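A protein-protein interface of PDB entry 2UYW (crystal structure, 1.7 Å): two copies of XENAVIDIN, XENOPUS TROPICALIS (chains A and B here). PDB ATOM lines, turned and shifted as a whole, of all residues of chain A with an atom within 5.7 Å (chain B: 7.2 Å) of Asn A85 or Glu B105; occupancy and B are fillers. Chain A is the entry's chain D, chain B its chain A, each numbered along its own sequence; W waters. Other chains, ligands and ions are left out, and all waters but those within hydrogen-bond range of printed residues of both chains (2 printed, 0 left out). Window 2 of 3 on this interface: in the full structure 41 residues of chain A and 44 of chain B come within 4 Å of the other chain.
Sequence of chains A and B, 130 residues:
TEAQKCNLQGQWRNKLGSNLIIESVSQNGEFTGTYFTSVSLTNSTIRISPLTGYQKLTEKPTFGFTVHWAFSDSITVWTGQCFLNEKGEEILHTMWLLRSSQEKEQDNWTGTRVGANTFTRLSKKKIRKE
No position is printed for both chains.
Of the 10 printed residues of chain A, 4 touch a printed residue of chain B. Hydrophobic or aromatic side chains of chain A within 4 Å of the printed part of chain B: Phe A83, Ile A91 and His A93.
OD1 of Asn A85 is in hydrogen-bond range of N of Glu A89. The side-chain carboxylate of Glu B103 is in salt-bridge range of the side-chain amino group of Lys B104. The backbone NH (N) of Ile A91 is in hydrogen-bond range of the backbone carbonyl oxygen (O) of Phe A83. OD1 of Asn A85 sits at hydrogen-bond distance from N of Lys A87 (2.9 Å). The side-chain amide oxygen of Asn A85 sits at hydrogen-bond distance from the backbone NH of Gly A88. The guanidinium group (NH2) of Arg B99 sits at hydrogen-bond distance from the side-chain amide oxygen (OD1) of Asn B108 (2.9 Å).
Among the printed residues, pairs that only touch across the chains: His A93 with Asn B108, Phe A83 with Asn B108, Phe A83 with Glu B105, Phe A83 with Lys B104, Ile A91 with Glu B105, Asn A85 with Glu B105, His A93 with Arg B99, Phe A83 with Gln B102 and Phe A83 with Arg B99.
Printed residues of chain A within 4 Å of Glu B105: Phe A83, Asn A85, Ile A91 and His A93. Of the printed residues of chain B, His A93 touches Arg B99, Glu B105 and Asn B108. Printed residues of chain B within 4 Å of Ile A91: Glu B105. Glu A89 touches none of the printed residues of chain B.
Water W1 lies within hydrogen-bond range of OE1 of Glu B105 (2.6 Å) and O of Leu A84 (2.7 Å). Water W2 bridges a ring nitrogen (NE2) of His A93 (3.3 Å) and the backbone carbonyl oxygen of Glu B105 (3.4 Å).
OE2 of Glu B105 sits at hydrogen-bond distance from NE2 of His A93, at 2.7 Å.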
ATOM      1  N   PHE A  83      26.610   8.710   1.628  1.00  0.00           N
ATOM      2  CA  PHE A  83      25.503   9.236   0.826  1.00  0.00           C
ATOM      3  C   PHE A  83      24.713  10.249   1.660  1.00  0.00           C
ATOM      4  O   PHE A  83      24.866  10.319   2.893  1.00  0.00           O
ATOM      5  CB  PHE A  83      24.564   8.088   0.435  1.00  0.00           C
ATOM      6  CG  PHE A  83      25.202   7.017  -0.402  1.00  0.00           C
ATOM      7  CD1 PHE A  83      25.267   7.145  -1.790  1.00  0.00           C
ATOM      8  CD2 PHE A  83      25.710   5.855   0.196  1.00  0.00           C
ATOM      9  CE1 PHE A  83      25.860   6.124  -2.585  1.00  0.00           C
ATOM     10  CE2 PHE A  83      26.306   4.833  -0.584  1.00  0.00           C
ATOM     11  CZ  PHE A  83      26.361   4.971  -1.972  1.00  0.00           C
ATOM     12  N   LEU A  84      23.874  11.047   1.001  1.00  0.00           N
ATOM     13  CA  LEU A  84      22.837  11.781   1.711  1.00  0.00           C
ATOM     14  C   LEU A  84      21.525  11.025   1.568  1.00  0.00           C
ATOM     15  O   LEU A  84      21.133  10.672   0.453  1.00  0.00           O
ATOM     16  CB  LEU A  84      22.693  13.201   1.161  1.00  0.00           C
ATOM     17  CG  LEU A  84      23.910  14.103   1.340  1.00  0.00           C
ATOM     18  CD1 LEU A  84      23.687  15.423   0.659  1.00  0.00           C
ATOM     19  CD2 LEU A  84      24.245  14.316   2.828  1.00  0.00           C
ATOM     20  N   ASN A  85      20.861  10.757   2.691  1.00  0.00           N
ATOM     21  CA  ASN A  85      19.557  10.085   2.673  1.00  0.00           C
ATOM     22  C   ASN A  85      18.431  11.022   2.212  1.00  0.00           C
ATOM     23  O   ASN A  85      18.687  12.154   1.778  1.00  0.00           O
ATOM     24  CB  ASN A  85      19.239   9.472   4.045  1.00  0.00           C
ATOM     25  CG  ASN A  85      18.879  10.527   5.102  1.00  0.00           C
ATOM     26  OD1 ASN A  85      18.780  11.723   4.818  1.00  0.00           O
ATOM     27  ND2 ASN A  85      18.700  10.073   6.334  1.00  0.00           N
ATOM     28  N   GLU A  86      17.188  10.545   2.316  1.00  0.00           N
ATOM     29  CA  GLU A  86      15.989  11.316   1.936  1.00  0.00           C
ATOM     30  C   GLU A  86      15.875  12.680   2.615  1.00  0.00           C
ATOM     31  O   GLU A  86      15.475  13.659   1.975  1.00  0.00           O
ATOM     32  CB  GLU A  86      14.703  10.518   2.217  1.00  0.00           C
ATOM     33  CG  GLU A  86      14.785   9.027   1.900  1.00  0.00           C
ATOM     34  CD  GLU A  86      13.436   8.318   2.003  1.00  0.00           C
ATOM     35  OE1 GLU A  86      13.436   7.110   2.357  1.00  0.00           O
ATOM     36  OE2 GLU A  86      12.388   8.954   1.726  1.00  0.00           O
ATOM     37  N   LYS A  87      16.212  12.737   3.906  1.00  0.00           N
ATOM     38  CA  LYS A  87      16.140  13.981   4.687  1.00  0.00           C
ATOM     39  C   LYS A  87      17.302  14.912   4.355  1.00  0.00           C
ATOM     40  O   LYS A  87      17.348  16.057   4.828  1.00  0.00           O
ATOM     41  CB  LYS A  87      16.156  13.693   6.196  1.00  0.00           C
ATOM     42  CG  LYS A  87      14.949  12.949   6.748  1.00  0.00           C
ATOM     43  CD  LYS A  87      15.245  11.466   6.902  1.00  0.00           C
ATOM     44  CE  LYS A  87      14.211  10.785   7.786  1.00  0.00           C
ATOM     45  NZ  LYS A  87      12.856  10.786   7.170  1.00  0.00           N
ATOM     46  N   GLY A  88      18.247  14.415   3.557  1.00  0.00           N
ATOM     47  CA  GLY A  88      19.454  15.165   3.233  1.00  0.00           C
ATOM     48  C   GLY A  88      20.503  15.063   4.331  1.00  0.00           C
ATOM     49  O   GLY A  88      21.393  15.906   4.420  1.00  0.00           O
ATOM     50  N   GLU A  89      20.395  14.029   5.168  1.00  0.00           N
ATOM     51  CA  GLU A  89      21.378  13.767   6.241  1.00  0.00           C
ATOM     52  C   GLU A  89      22.423  12.774   5.764  1.00  0.00           C
ATOM     53  O   GLU A  89      22.082  11.820   5.063  1.00  0.00           O
ATOM     54  CB  GLU A  89      20.702  13.164   7.474  1.00  0.00           C
ATOM     55  CG  GLU A  89      19.675  14.066   8.141  1.00  0.00           C
ATOM     56  CD  GLU A  89      18.740  13.291   9.039  1.00  0.00           C
ATOM     57  OE1 GLU A  89      18.598  12.066   8.837  1.00  0.00           O
ATOM     58  OE2 GLU A  89      18.132  13.906   9.941  1.00  0.00           O
ATOM     59  N   GLU A  90      23.669  12.983   6.194  1.00  0.00           N
ATOM     60  CA  GLU A  90      24.811  12.139   5.828  1.00  0.00           C
ATOM     61  C   GLU A  90      24.735  10.763   6.476  1.00  0.00           C
ATOM     62  O   GLU A  90      24.419  10.630   7.662  1.00  0.00           O
ATOM     63  CB  GLU A  90      26.120  12.743   6.319  1.00  0.00           C
ATOM     64  CG  GLU A  90      26.472  14.107   5.819  1.00  0.00           C
ATOM     65  CD  GLU A  90      27.469  14.783   6.750  1.00  0.00           C
ATOM     66  OE1 GLU A  90      27.111  15.046   7.925  1.00  0.00           O
ATOM     67  OE2 GLU A  90      28.608  15.047   6.316  1.00  0.00           O
ATOM     68  N   ILE A  91      25.063   9.742   5.692  1.00  0.00           N
ATOM     69  CA  ILE A  91      25.052   8.386   6.201  1.00  0.00           C
ATOM     70  C   ILE A  91      26.227   7.618   5.637  1.00  0.00           C
ATOM     71  O   ILE A  91      26.504   7.687   4.436  1.00  0.00           O
ATOM     72  CB  ILE A  91      23.721   7.662   5.886  1.00  0.00           C
ATOM     73  CG1 ILE A  91      23.702   6.260   6.469  1.00  0.00           C
ATOM     74  CG2 ILE A  91      23.410   7.676   4.365  1.00  0.00           C
ATOM     75  CD1 ILE A  91      22.270   5.790   6.711  1.00  0.00           C
ATOM     76  N   HIS A  93      27.506   4.007   4.866  1.00  0.00           N
ATOM     77  CA  HIS A  93      27.166   2.607   4.771  1.00  0.00           C
ATOM     78  C   HIS A  93      28.470   1.832   4.713  1.00  0.00           C
ATOM     79  O   HIS A  93      29.282   2.066   3.804  1.00  0.00           O
ATOM     80  CB  HIS A  93      26.351   2.346   3.498  1.00  0.00           C
ATOM     81  CG  HIS A  93      24.952   2.872   3.569  1.00  0.00           C
ATOM     82  ND1 HIS A  93      24.035   2.416   4.494  1.00  0.00           N
ATOM     83  CD2 HIS A  93      24.311   3.811   2.834  1.00  0.00           C
ATOM     84  CE1 HIS A  93      22.889   3.050   4.315  1.00  0.00           C
ATOM     85  NE2 HIS A  93      23.031   3.902   3.319  1.00  0.00           N
ATOM     86  N   ARG B  99      35.511  -2.096  -1.808  1.00  0.00           N
ATOM     87  CA  ARG B  99      34.375  -1.178  -1.991  1.00  0.00           C
ATOM     88  C   ARG B  99      34.465  -0.494  -3.326  1.00  0.00           C
ATOM     89  O   ARG B  99      35.442   0.202  -3.620  1.00  0.00           O
ATOM     90  CB  ARG B  99      34.361  -0.087  -0.900  1.00  0.00           C
ATOM     91  CG  ARG B  99      33.260   0.963  -1.152  1.00  0.00           C
ATOM     92  CD  ARG B  99      31.892   0.314  -0.802  1.00  0.00           C
ATOM     93  NE  ARG B  99      30.792   1.024  -1.438  1.00  0.00           N
ATOM     94  CZ  ARG B  99      29.553   1.057  -0.958  1.00  0.00           C
ATOM     95  NH1 ARG B  99      29.244   0.493   0.213  1.00  0.00           N
ATOM     96  NH2 ARG B  99      28.607   1.681  -1.645  1.00  0.00           N
ATOM     97  N   GLN B 102      29.404   3.494  -5.859  1.00  0.00           N
ATOM     98  CA  GLN B 102      28.083   3.458  -6.489  1.00  0.00           C
ATOM     99  C   GLN B 102      27.531   4.848  -6.750  1.00  0.00           C
ATOM    100  O   GLN B 102      27.845   5.812  -6.038  1.00  0.00           O
ATOM    101  CB  GLN B 102      27.084   2.664  -5.621  1.00  0.00           C
ATOM    102  CG  GLN B 102      27.533   1.240  -5.306  1.00  0.00           C
ATOM    103  CD  GLN B 102      27.921   0.463  -6.549  1.00  0.00           C
ATOM    104  OE1 GLN B 102      27.141   0.370  -7.508  1.00  0.00           O
ATOM    105  NE2 GLN B 102      29.134  -0.090  -6.551  1.00  0.00           N
ATOM    106  N   GLU B 103      26.697   4.960  -7.776  1.00  0.00           N
ATOM    107  CA  GLU B 103      26.136   6.268  -8.122  1.00  0.00           C
ATOM    108  C   GLU B 103      24.994   6.685  -7.191  1.00  0.00           C
ATOM    109  O   GLU B 103      24.773   7.874  -6.981  1.00  0.00           O
ATOM    110  CB  GLU B 103      25.710   6.352  -9.607  1.00  0.00           C
ATOM    111  CG  GLU B 103      25.127   5.058 -10.165  1.00  0.00           C
ATOM    112  CD  GLU B 103      24.201   5.261 -11.378  1.00  0.00           C
ATOM    113  OE1 GLU B 103      24.402   6.221 -12.165  1.00  0.00           O
ATOM    114  OE2 GLU B 103      23.256   4.445 -11.544  1.00  0.00           O
ATOM    115  N   LYS B 104      24.279   5.724  -6.621  1.00  0.00           N
ATOM    116  CA  LYS B 104      23.077   6.040  -5.844  1.00  0.00           C
ATOM    117  C   LYS B 104      23.021   5.187  -4.595  1.00  0.00           C
ATOM    118  O   LYS B 104      23.463   4.049  -4.627  1.00  0.00           O
ATOM    119  CB  LYS B 104      21.825   5.726  -6.665  1.00  0.00           C
ATOM    120  CG  LYS B 104      21.508   6.676  -7.799  1.00  0.00           C
ATOM    121  CD  LYS B 104      20.264   6.180  -8.531  1.00  0.00           C
ATOM    122  CE  LYS B 104      20.603   5.099  -9.555  1.00  0.00           C
ATOM    123  NZ  LYS B 104      20.577   3.716  -9.012  1.00  0.00           N
ATOM    124  N   GLU B 105      22.446   5.727  -3.520  1.00  0.00           N
ATOM    125  CA  GLU B 105      22.319   5.008  -2.244  1.00  0.00           C
ATOM    126  C   GLU B 105      21.565   3.689  -2.411  1.00  0.00           C
ATOM    127  O   GLU B 105      21.842   2.694  -1.716  1.00  0.00           O
ATOM    128  CB  GLU B 105      21.623   5.880  -1.178  1.00  0.00           C
ATOM    129  CG  GLU B 105      21.827   5.313   0.245  1.00  0.00           C
ATOM    130  CD  GLU B 105      20.910   5.903   1.322  1.00  0.00           C
ATOM    131  OE1 GLU B 105      20.033   6.765   1.022  1.00  0.00           O
ATOM    132  OE2 GLU B 105      21.063   5.492   2.493  1.00  0.00           O
ATOM    133  N   GLN B 106      20.624   3.680  -3.351  1.00  0.00           N
ATOM    134  CA  GLN B 106      19.791   2.496  -3.603  1.00  0.00           C
ATOM    135  C   GLN B 106      20.598   1.303  -4.128  1.00  0.00           C
ATOM    136  O   GLN B 106      20.141   0.144  -4.038  1.00  0.00           O
ATOM    137  CB  GLN B 106      18.600   2.824  -4.531  1.00  0.00           C
ATOM    138  CG  GLN B 106      18.945   3.104  -5.995  1.00  0.00           C
ATOM    139  CD  GLN B 106      17.709   3.438  -6.837  1.00  0.00           C
ATOM    140  OE1 GLN B 106      17.178   4.551  -6.781  1.00  0.00           O
ATOM    141  NE2 GLN B 106      17.253   2.470  -7.627  1.00  0.00           N
ATOM    142  N   ASP B 107      21.785   1.569  -4.663  1.00  0.00           N
ATOM    143  CA  ASP B 107      22.665   0.529  -5.201  1.00  0.00           C
ATOM    144  C   ASP B 107      23.746   0.105  -4.214  1.00  0.00           C
ATOM    145  O   ASP B 107      24.643  -0.659  -4.557  1.00  0.00           O
ATOM    146  CB  ASP B 107      23.322   0.994  -6.499  1.00  0.00           C
ATOM    147  CG  ASP B 107      22.328   1.142  -7.631  1.00  0.00           C
ATOM    148  OD1 ASP B 107      21.237   0.526  -7.586  1.00  0.00           O
ATOM    149  OD2 ASP B 107      22.664   1.861  -8.579  1.00  0.00           O
ATOM    150  N   ASN B 108      23.665   0.598  -2.978  1.00  0.00           N
ATOM    151  CA  ASN B 108      24.703   0.332  -2.006  1.00  0.00           C
ATOM    152  C   ASN B 108      24.953  -1.166  -1.776  1.00  0.00           C
ATOM    153  O   ASN B 108      26.101  -1.571  -1.597  1.00  0.00           O
ATOM    154  CB  ASN B 108      24.359   0.994  -0.656  1.00  0.00           C
ATOM    155  CG  ASN B 108      25.455   0.794   0.372  1.00  0.00           C
ATOM    156  OD1 ASN B 108      26.507   1.414   0.283  1.00  0.00           O
ATOM    157  ND2 ASN B 108      25.230  -0.102   1.322  1.00  0.00           N
ATOM    158  N   TRP B 109      23.875  -1.954  -1.822  1.00  0.00           N
ATOM    159  CA  TRP B 109      23.954  -3.389  -1.539  1.00  0.00           C
ATOM    160  C   TRP B 109      24.887  -4.096  -2.512  1.00  0.00           C
ATOM    161  O   TRP B 109      25.364  -5.179  -2.198  1.00  0.00           O
ATOM    162  CB  TRP B 109      22.560  -4.002  -1.636  1.00  0.00           C
ATOM    163  CG  TRP B 109      21.976  -4.004  -3.026  1.00  0.00           C
ATOM    164  CD1 TRP B 109      21.232  -3.010  -3.625  1.00  0.00           C
ATOM    165  CD2 TRP B 109      22.105  -5.055  -3.993  1.00  0.00           C
ATOM    166  NE1 TRP B 109      20.862  -3.409  -4.914  1.00  0.00           N
ATOM    167  CE2 TRP B 109      21.405  -4.651  -5.158  1.00  0.00           C
ATOM    168  CE3 TRP B 109      22.752  -6.307  -3.983  1.00  0.00           C
ATOM    169  CZ2 TRP B 109      21.321  -5.471  -6.312  1.00  0.00           C
ATOM    170  CZ3 TRP B 109      22.688  -7.107  -5.140  1.00  0.00           C
ATOM    171  CH2 TRP B 109      21.964  -6.695  -6.270  1.00  0.00           C
HETATM  172  O   HOH W   1      19.495   8.812  -0.524  1.00  0.00           O
HETATM  173  O   HOH W   2      21.185   1.916   1.492  1.00  0.00           O
